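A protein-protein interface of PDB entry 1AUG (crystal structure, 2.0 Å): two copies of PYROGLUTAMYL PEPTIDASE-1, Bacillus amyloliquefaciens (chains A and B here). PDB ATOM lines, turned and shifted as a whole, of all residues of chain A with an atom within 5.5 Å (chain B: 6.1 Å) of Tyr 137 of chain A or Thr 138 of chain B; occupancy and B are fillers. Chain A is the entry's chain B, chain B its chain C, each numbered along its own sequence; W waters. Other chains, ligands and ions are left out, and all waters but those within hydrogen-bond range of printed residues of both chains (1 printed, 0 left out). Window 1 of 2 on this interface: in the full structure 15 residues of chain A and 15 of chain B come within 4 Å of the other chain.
NH2 of Arg 82 of chain A lies within salt-bridge range of OE1 of Glu 89 of chain B.
O of Thr 138 of chain B is in hydrogen-bond range of OG of Ser 136 of chain B, at 3.0 Å.
The guanidinium group of Arg 82 of chain B sits at hydrogen-bond distance from the side-chain hydroxyl of Tyr 137 of chain B (3.0 Å).
The side-chain hydroxyl of Thr 138 of chain B lies within hydrogen-bond range of the backbone NH of Gly 140 of chain B.
O of Thr 138 of chain A lies within hydrogen-bond range of OG of Ser 136 of chain A.
The guanidinium group (NH1) of Arg 82 of chain A is in hydrogen-bond range of the side-chain hydroxyl (OH) of Tyr 137 of chain A (3.1 Å).
O of Glu 89 of chain B is in hydrogen-bond range of OG1 of Thr 141 of chain B (2.9 Å).
Among the printed residues, merely in contact across the chains: Tyr 137 of chain A with Leu 87 of chain B, Tyr 137 of chain A with Glu 89 of chain B, Tyr 137 of chain A with Thr 138 of chain B, Tyr 137 of chain A with Thr 141 of chain B, Thr 138 of chain A with Tyr 137 of chain B and Thr 138 of chain A with Thr 138 of chain B.
Printed residues of chain B within 4 Å of Arg 82 of chain A: Glu 89.
Printed residues of chain B within 4 Å of Thr 138 of chain A: Tyr 137 (3.8 Å) and Thr 138 (3.4 Å).
Ala 139 of chain A touches none of the printed residues of chain B.
Arg 82 of chain B touches none of the printed residues of chain A.
Of the printed residues of chain A, Glu 89 of chain B touches Arg 82 and Tyr 137.
Of the printed residues of chain A, Tyr 137 of chain B touches Thr 138.
Printed residues of chain A within 4 Å of Thr 138 of chain B: Tyr 137 and Thr 138.
Printed residues of chain A within 4 Å of Thr 141 of chain B: Tyr 137.
The nearest residue of chain B that does not touch Tyr 137 of chain A is Tyr 137 of chain B (4.4 Å).
The nearest printed residue of chain B that does not touch Arg 82 of chain A is Leu 87 of chain B (4.1 Å).
Of the 8 printed residues of chain A, 3 touch a printed residue of chain B.
Hydrophobic or aromatic side chains of chain A that line the printed part of chain B: Tyr 137.
Tyr 137 of chain A touches Thr 138 of chain B, and with the chains exchanged Thr 138 of chain A touches Tyr 137 of chain B.
Thr 138 of chain A touches its own counterpart, Thr 138 of chain B.
7 positions are printed for both chains.
Water W1 lies within hydrogen-bond range of the backbone carbonyl oxygen (O) of Tyr 137 of chain A (2.7 Å) and the backbone carbonyl oxygen (O) of Tyr 137 of chain B (2.9 Å).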
ATOM      1  N   GLU A  81      25.627  -4.609 -17.680  1.00  0.00           N
ATOM      2  CA  GLU A  81      24.358  -5.230 -17.266  1.00  0.00           C
ATOM      3  C   GLU A  81      23.146  -4.372 -17.556  1.00  0.00           C
ATOM      4  O   GLU A  81      23.224  -3.196 -17.208  1.00  0.00           O
ATOM      5  CB  GLU A  81      24.451  -5.507 -15.811  1.00  0.00           C
ATOM      6  CG  GLU A  81      25.566  -6.482 -15.488  1.00  0.00           C
ATOM      7  CD  GLU A  81      25.335  -7.892 -16.006  1.00  0.00           C
ATOM      8  OE1 GLU A  81      24.252  -8.231 -16.478  1.00  0.00           O
ATOM      9  OE2 GLU A  81      26.233  -8.702 -15.890  1.00  0.00           O
ATOM     10  N   ARG A  82      22.073  -4.841 -18.202  1.00  0.00           N
ATOM     11  CA  ARG A  82      20.891  -4.038 -18.450  1.00  0.00           C
ATOM     12  C   ARG A  82      19.979  -4.009 -17.236  1.00  0.00           C
ATOM     13  O   ARG A  82      19.317  -2.986 -17.086  1.00  0.00           O
ATOM     14  CB  ARG A  82      20.088  -4.590 -19.633  1.00  0.00           C
ATOM     15  CG  ARG A  82      18.953  -3.707 -20.264  1.00  0.00           C
ATOM     16  CD  ARG A  82      19.591  -2.843 -21.333  1.00  0.00           C
ATOM     17  NE  ARG A  82      18.772  -2.240 -22.366  1.00  0.00           N
ATOM     18  CZ  ARG A  82      18.723  -2.678 -23.657  1.00  0.00           C
ATOM     19  NH1 ARG A  82      19.433  -3.704 -24.141  1.00  0.00           N
ATOM     20  NH2 ARG A  82      17.928  -2.049 -24.541  1.00  0.00           N
ATOM     21  N   VAL A  83      19.927  -4.989 -16.333  1.00  0.00           N
ATOM     22  CA  VAL A  83      18.871  -5.136 -15.311  1.00  0.00           C
ATOM     23  C   VAL A  83      19.357  -5.574 -13.954  1.00  0.00           C
ATOM     24  O   VAL A  83      20.026  -6.619 -13.912  1.00  0.00           O
ATOM     25  CB  VAL A  83      17.754  -6.246 -15.576  1.00  0.00           C
ATOM     26  CG1 VAL A  83      16.433  -5.581 -15.213  1.00  0.00           C
ATOM     27  CG2 VAL A  83      17.694  -6.809 -16.956  1.00  0.00           C
ATOM     28  N   VAL A 135      25.935  -6.890 -24.186  1.00  0.00           N
ATOM     29  CA  VAL A 135      25.097  -6.625 -23.027  1.00  0.00           C
ATOM     30  C   VAL A 135      24.509  -7.945 -22.489  1.00  0.00           C
ATOM     31  O   VAL A 135      24.218  -8.937 -23.170  1.00  0.00           O
ATOM     32  CB  VAL A 135      23.979  -5.463 -23.329  1.00  0.00           C
ATOM     33  CG1 VAL A 135      23.846  -5.113 -24.747  1.00  0.00           C
ATOM     34  CG2 VAL A 135      22.620  -5.842 -22.781  1.00  0.00           C
ATOM     35  N   SER A 136      24.552  -7.992 -21.179  1.00  0.00           N
ATOM     36  CA  SER A 136      24.002  -9.074 -20.397  1.00  0.00           C
ATOM     37  C   SER A 136      22.661  -8.653 -19.761  1.00  0.00           C
ATOM     38  O   SER A 136      22.501  -7.473 -19.341  1.00  0.00           O
ATOM     39  CB  SER A 136      24.983  -9.414 -19.340  1.00  0.00           C
ATOM     40  OG  SER A 136      24.417 -10.259 -18.343  1.00  0.00           O
ATOM     41  N   TYR A 137      21.740  -9.637 -19.588  1.00  0.00           N
ATOM     42  CA  TYR A 137      20.443  -9.376 -18.998  1.00  0.00           C
ATOM     43  C   TYR A 137      20.288 -10.082 -17.670  1.00  0.00           C
ATOM     44  O   TYR A 137      19.184 -10.141 -17.151  1.00  0.00           O
ATOM     45  CB  TYR A 137      19.340  -9.805 -19.948  1.00  0.00           C
ATOM     46  CG  TYR A 137      19.377  -8.984 -21.219  1.00  0.00           C
ATOM     47  CD1 TYR A 137      18.673  -7.786 -21.304  1.00  0.00           C
ATOM     48  CD2 TYR A 137      20.122  -9.414 -22.320  1.00  0.00           C
ATOM     49  CE1 TYR A 137      18.723  -7.029 -22.481  1.00  0.00           C
ATOM     50  CE2 TYR A 137      20.163  -8.662 -23.488  1.00  0.00           C
ATOM     51  CZ  TYR A 137      19.458  -7.474 -23.565  1.00  0.00           C
ATOM     52  OH  TYR A 137      19.467  -6.739 -24.746  1.00  0.00           O
ATOM     53  N   THR A 138      21.293 -10.674 -17.060  1.00  0.00           N
ATOM     54  CA  THR A 138      21.171 -11.049 -15.656  1.00  0.00           C
ATOM     55  C   THR A 138      22.527 -10.829 -15.022  1.00  0.00           C
ATOM     56  O   THR A 138      23.544 -11.288 -15.562  1.00  0.00           O
ATOM     57  CB  THR A 138      20.722 -12.541 -15.473  1.00  0.00           C
ATOM     58  OG1 THR A 138      21.001 -12.877 -14.100  1.00  0.00           O
ATOM     59  CG2 THR A 138      21.451 -13.560 -16.302  1.00  0.00           C
ATOM     60  N   ALA A 139      22.578 -10.180 -13.877  1.00  0.00           N
ATOM     61  CA  ALA A 139      23.792  -9.983 -13.158  1.00  0.00           C
ATOM     62  C   ALA A 139      23.912 -10.925 -11.982  1.00  0.00           C
ATOM     63  O   ALA A 139      24.777 -10.757 -11.129  1.00  0.00           O
ATOM     64  CB  ALA A 139      23.854  -8.561 -12.693  1.00  0.00           C
ATOM     65  N   ARG B  75      20.276 -24.961 -23.773  1.00  0.00           N
ATOM     66  CA  ARG B  75      20.371 -25.307 -22.349  1.00  0.00           C
ATOM     67  C   ARG B  75      20.301 -26.836 -22.196  1.00  0.00           C
ATOM     68  O   ARG B  75      19.892 -27.563 -23.120  1.00  0.00           O
ATOM     69  CB  ARG B  75      19.237 -24.594 -21.522  1.00  0.00           C
ATOM     70  CG  ARG B  75      18.847 -23.261 -22.168  1.00  0.00           C
ATOM     71  CD  ARG B  75      18.930 -21.939 -21.452  1.00  0.00           C
ATOM     72  NE  ARG B  75      17.835 -21.727 -20.569  1.00  0.00           N
ATOM     73  CZ  ARG B  75      17.243 -20.549 -20.343  1.00  0.00           C
ATOM     74  NH1 ARG B  75      17.530 -19.360 -20.882  1.00  0.00           N
ATOM     75  NH2 ARG B  75      16.317 -20.621 -19.423  1.00  0.00           N
ATOM     76  N   GLU B  81      11.449 -19.963 -15.230  1.00  0.00           N
ATOM     77  CA  GLU B  81      11.953 -18.592 -15.232  1.00  0.00           C
ATOM     78  C   GLU B  81      11.588 -17.787 -14.011  1.00  0.00           C
ATOM     79  O   GLU B  81      10.410 -17.826 -13.707  1.00  0.00           O
ATOM     80  CB  GLU B  81      11.431 -17.908 -16.489  1.00  0.00           C
ATOM     81  CG  GLU B  81      11.976 -18.545 -17.746  1.00  0.00           C
ATOM     82  CD  GLU B  81      13.506 -18.469 -17.904  1.00  0.00           C
ATOM     83  OE1 GLU B  81      14.186 -17.770 -17.179  1.00  0.00           O
ATOM     84  OE2 GLU B  81      14.054 -19.104 -18.792  1.00  0.00           O
ATOM     85  N   ARG B  82      12.480 -17.119 -13.244  1.00  0.00           N
ATOM     86  CA  ARG B  82      12.057 -16.309 -12.128  1.00  0.00           C
ATOM     87  C   ARG B  82      11.583 -14.911 -12.569  1.00  0.00           C
ATOM     88  O   ARG B  82      10.735 -14.385 -11.861  1.00  0.00           O
ATOM     89  CB  ARG B  82      13.188 -16.120 -11.115  1.00  0.00           C
ATOM     90  CG  ARG B  82      12.862 -15.523  -9.734  1.00  0.00           C
ATOM     91  CD  ARG B  82      12.476 -16.691  -8.864  1.00  0.00           C
ATOM     92  NE  ARG B  82      12.622 -16.642  -7.413  1.00  0.00           N
ATOM     93  CZ  ARG B  82      13.651 -17.185  -6.692  1.00  0.00           C
ATOM     94  NH1 ARG B  82      14.703 -17.851  -7.203  1.00  0.00           N
ATOM     95  NH2 ARG B  82      13.655 -17.053  -5.358  1.00  0.00           N
ATOM     96  N   VAL B  83      12.004 -14.305 -13.702  1.00  0.00           N
ATOM     97  CA  VAL B  83      11.809 -12.894 -14.022  1.00  0.00           C
ATOM     98  C   VAL B  83      11.506 -12.632 -15.466  1.00  0.00           C
ATOM     99  O   VAL B  83      12.256 -13.088 -16.355  1.00  0.00           O
ATOM    100  CB  VAL B  83      13.026 -11.950 -13.814  1.00  0.00           C
ATOM    101  CG1 VAL B  83      12.480 -10.664 -13.269  1.00  0.00           C
ATOM    102  CG2 VAL B  83      14.055 -12.482 -12.880  1.00  0.00           C
ATOM    103  N   ILE B  85      10.922  -9.391 -18.218  1.00  0.00           N
ATOM    104  CA  ILE B  85      11.511  -8.068 -18.302  1.00  0.00           C
ATOM    105  C   ILE B  85      10.710  -7.300 -19.321  1.00  0.00           C
ATOM    106  O   ILE B  85      10.263  -7.854 -20.304  1.00  0.00           O
ATOM    107  CB  ILE B  85      13.035  -8.417 -18.614  1.00  0.00           C
ATOM    108  CG1 ILE B  85      13.696  -7.838 -17.481  1.00  0.00           C
ATOM    109  CG2 ILE B  85      13.689  -7.953 -19.881  1.00  0.00           C
ATOM    110  CD1 ILE B  85      13.927  -8.899 -16.462  1.00  0.00           C
ATOM    111  N   LEU B  87      10.828  -5.625 -22.148  1.00  0.00           N
ATOM    112  CA  LEU B  87      11.646  -5.187 -23.264  1.00  0.00           C
ATOM    113  C   LEU B  87      11.470  -6.178 -24.377  1.00  0.00           C
ATOM    114  O   LEU B  87      11.537  -7.369 -24.103  1.00  0.00           O
ATOM    115  CB  LEU B  87      13.102  -5.184 -22.813  1.00  0.00           C
ATOM    116  CG  LEU B  87      14.251  -4.299 -23.388  1.00  0.00           C
ATOM    117  CD1 LEU B  87      15.454  -5.189 -23.430  1.00  0.00           C
ATOM    118  CD2 LEU B  87      14.001  -3.734 -24.750  1.00  0.00           C
ATOM    119  N   GLU B  89      13.532  -7.041 -27.692  1.00  0.00           N
ATOM    120  CA  GLU B  89      14.817  -6.735 -28.312  1.00  0.00           C
ATOM    121  C   GLU B  89      15.137  -7.971 -29.160  1.00  0.00           C
ATOM    122  O   GLU B  89      15.633  -9.003 -28.694  1.00  0.00           O
ATOM    123  CB  GLU B  89      15.790  -6.547 -27.213  1.00  0.00           C
ATOM    124  CG  GLU B  89      17.205  -6.237 -27.622  1.00  0.00           C
ATOM    125  CD  GLU B  89      17.545  -4.777 -27.869  1.00  0.00           C
ATOM    126  OE1 GLU B  89      17.252  -3.882 -27.064  1.00  0.00           O
ATOM    127  OE2 GLU B  89      18.183  -4.551 -28.879  1.00  0.00           O
ATOM    128  N   SER B 136      16.192 -20.328 -13.851  1.00  0.00           N
ATOM    129  CA  SER B 136      16.855 -19.383 -14.711  1.00  0.00           C
ATOM    130  C   SER B 136      16.431 -17.992 -14.318  1.00  0.00           C
ATOM    131  O   SER B 136      15.287 -17.801 -13.896  1.00  0.00           O
ATOM    132  CB  SER B 136      16.446 -19.728 -16.095  1.00  0.00           C
ATOM    133  OG  SER B 136      16.712 -18.763 -17.070  1.00  0.00           O
ATOM    134  N   TYR B 137      17.308 -17.004 -14.506  1.00  0.00           N
ATOM    135  CA  TYR B 137      17.022 -15.635 -14.173  1.00  0.00           C
ATOM    136  C   TYR B 137      16.984 -14.726 -15.383  1.00  0.00           C
ATOM    137  O   TYR B 137      17.013 -13.494 -15.228  1.00  0.00           O
ATOM    138  CB  TYR B 137      18.049 -15.120 -13.168  1.00  0.00           C
ATOM    139  CG  TYR B 137      17.903 -15.841 -11.825  1.00  0.00           C
ATOM    140  CD1 TYR B 137      16.980 -15.414 -10.843  1.00  0.00           C
ATOM    141  CD2 TYR B 137      18.703 -16.963 -11.580  1.00  0.00           C
ATOM    142  CE1 TYR B 137      16.874 -16.113  -9.633  1.00  0.00           C
ATOM    143  CE2 TYR B 137      18.594 -17.658 -10.389  1.00  0.00           C
ATOM    144  CZ  TYR B 137      17.683 -17.240  -9.421  1.00  0.00           C
ATOM    145  OH  TYR B 137      17.566 -17.964  -8.241  1.00  0.00           O
ATOM    146  N   THR B 138      16.994 -15.251 -16.619  1.00  0.00           N
ATOM    147  CA  THR B 138      16.728 -14.416 -17.780  1.00  0.00           C
ATOM    148  C   THR B 138      16.034 -15.308 -18.772  1.00  0.00           C
ATOM    149  O   THR B 138      16.396 -16.459 -18.976  1.00  0.00           O
ATOM    150  CB  THR B 138      18.050 -13.795 -18.371  1.00  0.00           C
ATOM    151  OG1 THR B 138      17.611 -13.192 -19.575  1.00  0.00           O
ATOM    152  CG2 THR B 138      19.214 -14.738 -18.638  1.00  0.00           C
ATOM    153  N   ALA B 139      14.944 -14.833 -19.343  1.00  0.00           N
ATOM    154  CA  ALA B 139      14.192 -15.580 -20.311  1.00  0.00           C
ATOM    155  C   ALA B 139      14.447 -15.013 -21.683  1.00  0.00           C
ATOM    156  O   ALA B 139      13.778 -15.347 -22.664  1.00  0.00           O
ATOM    157  CB  ALA B 139      12.698 -15.496 -19.932  1.00  0.00           C
ATOM    158  N   GLY B 140      15.521 -14.238 -21.845  1.00  0.00           N
ATOM    159  CA  GLY B 140      15.780 -13.645 -23.151  1.00  0.00           C
ATOM    160  C   GLY B 140      14.996 -12.334 -23.369  1.00  0.00           C
ATOM    161  O   GLY B 140      14.433 -11.770 -22.447  1.00  0.00           O
ATOM    162  N   THR B 141      14.930 -11.817 -24.593  1.00  0.00           N
ATOM    163  CA  THR B 141      14.236 -10.593 -24.896  1.00  0.00           C
ATOM    164  C   THR B 141      13.464 -10.799 -26.190  1.00  0.00           C
ATOM    165  O   THR B 141      13.050  -9.839 -26.832  1.00  0.00           O
ATOM    166  CB  THR B 141      15.256  -9.447 -25.040  1.00  0.00           C
ATOM    167  OG1 THR B 141      16.200  -9.880 -25.994  1.00  0.00           O
ATOM    168  CG2 THR B 141      15.990  -9.108 -23.781  1.00  0.00           C
ATOM    169  N   HIS B 168      11.192 -22.748 -19.661  1.00  0.00           N
ATOM    170  CA  HIS B 168      11.946 -22.954 -20.905  1.00  0.00           C
ATOM    171  C   HIS B 168      12.426 -24.429 -20.904  1.00  0.00           C
ATOM    172  O   HIS B 168      12.722 -25.014 -19.849  1.00  0.00           O
ATOM    173  CB  HIS B 168      13.157 -22.017 -20.951  1.00  0.00           C
ATOM    174  CG  HIS B 168      12.970 -20.797 -21.811  1.00  0.00           C
ATOM    175  ND1 HIS B 168      13.185 -19.516 -21.513  1.00  0.00           N
ATOM    176  CD2 HIS B 168      12.543 -20.843 -23.113  1.00  0.00           C
ATOM    177  CE1 HIS B 168      12.926 -18.805 -22.581  1.00  0.00           C
ATOM    178  NE2 HIS B 168      12.542 -19.623 -23.530  1.00  0.00           N
HETATM  179  O   HOH W   1      16.853 -10.669 -15.975  1.00  0.00           O
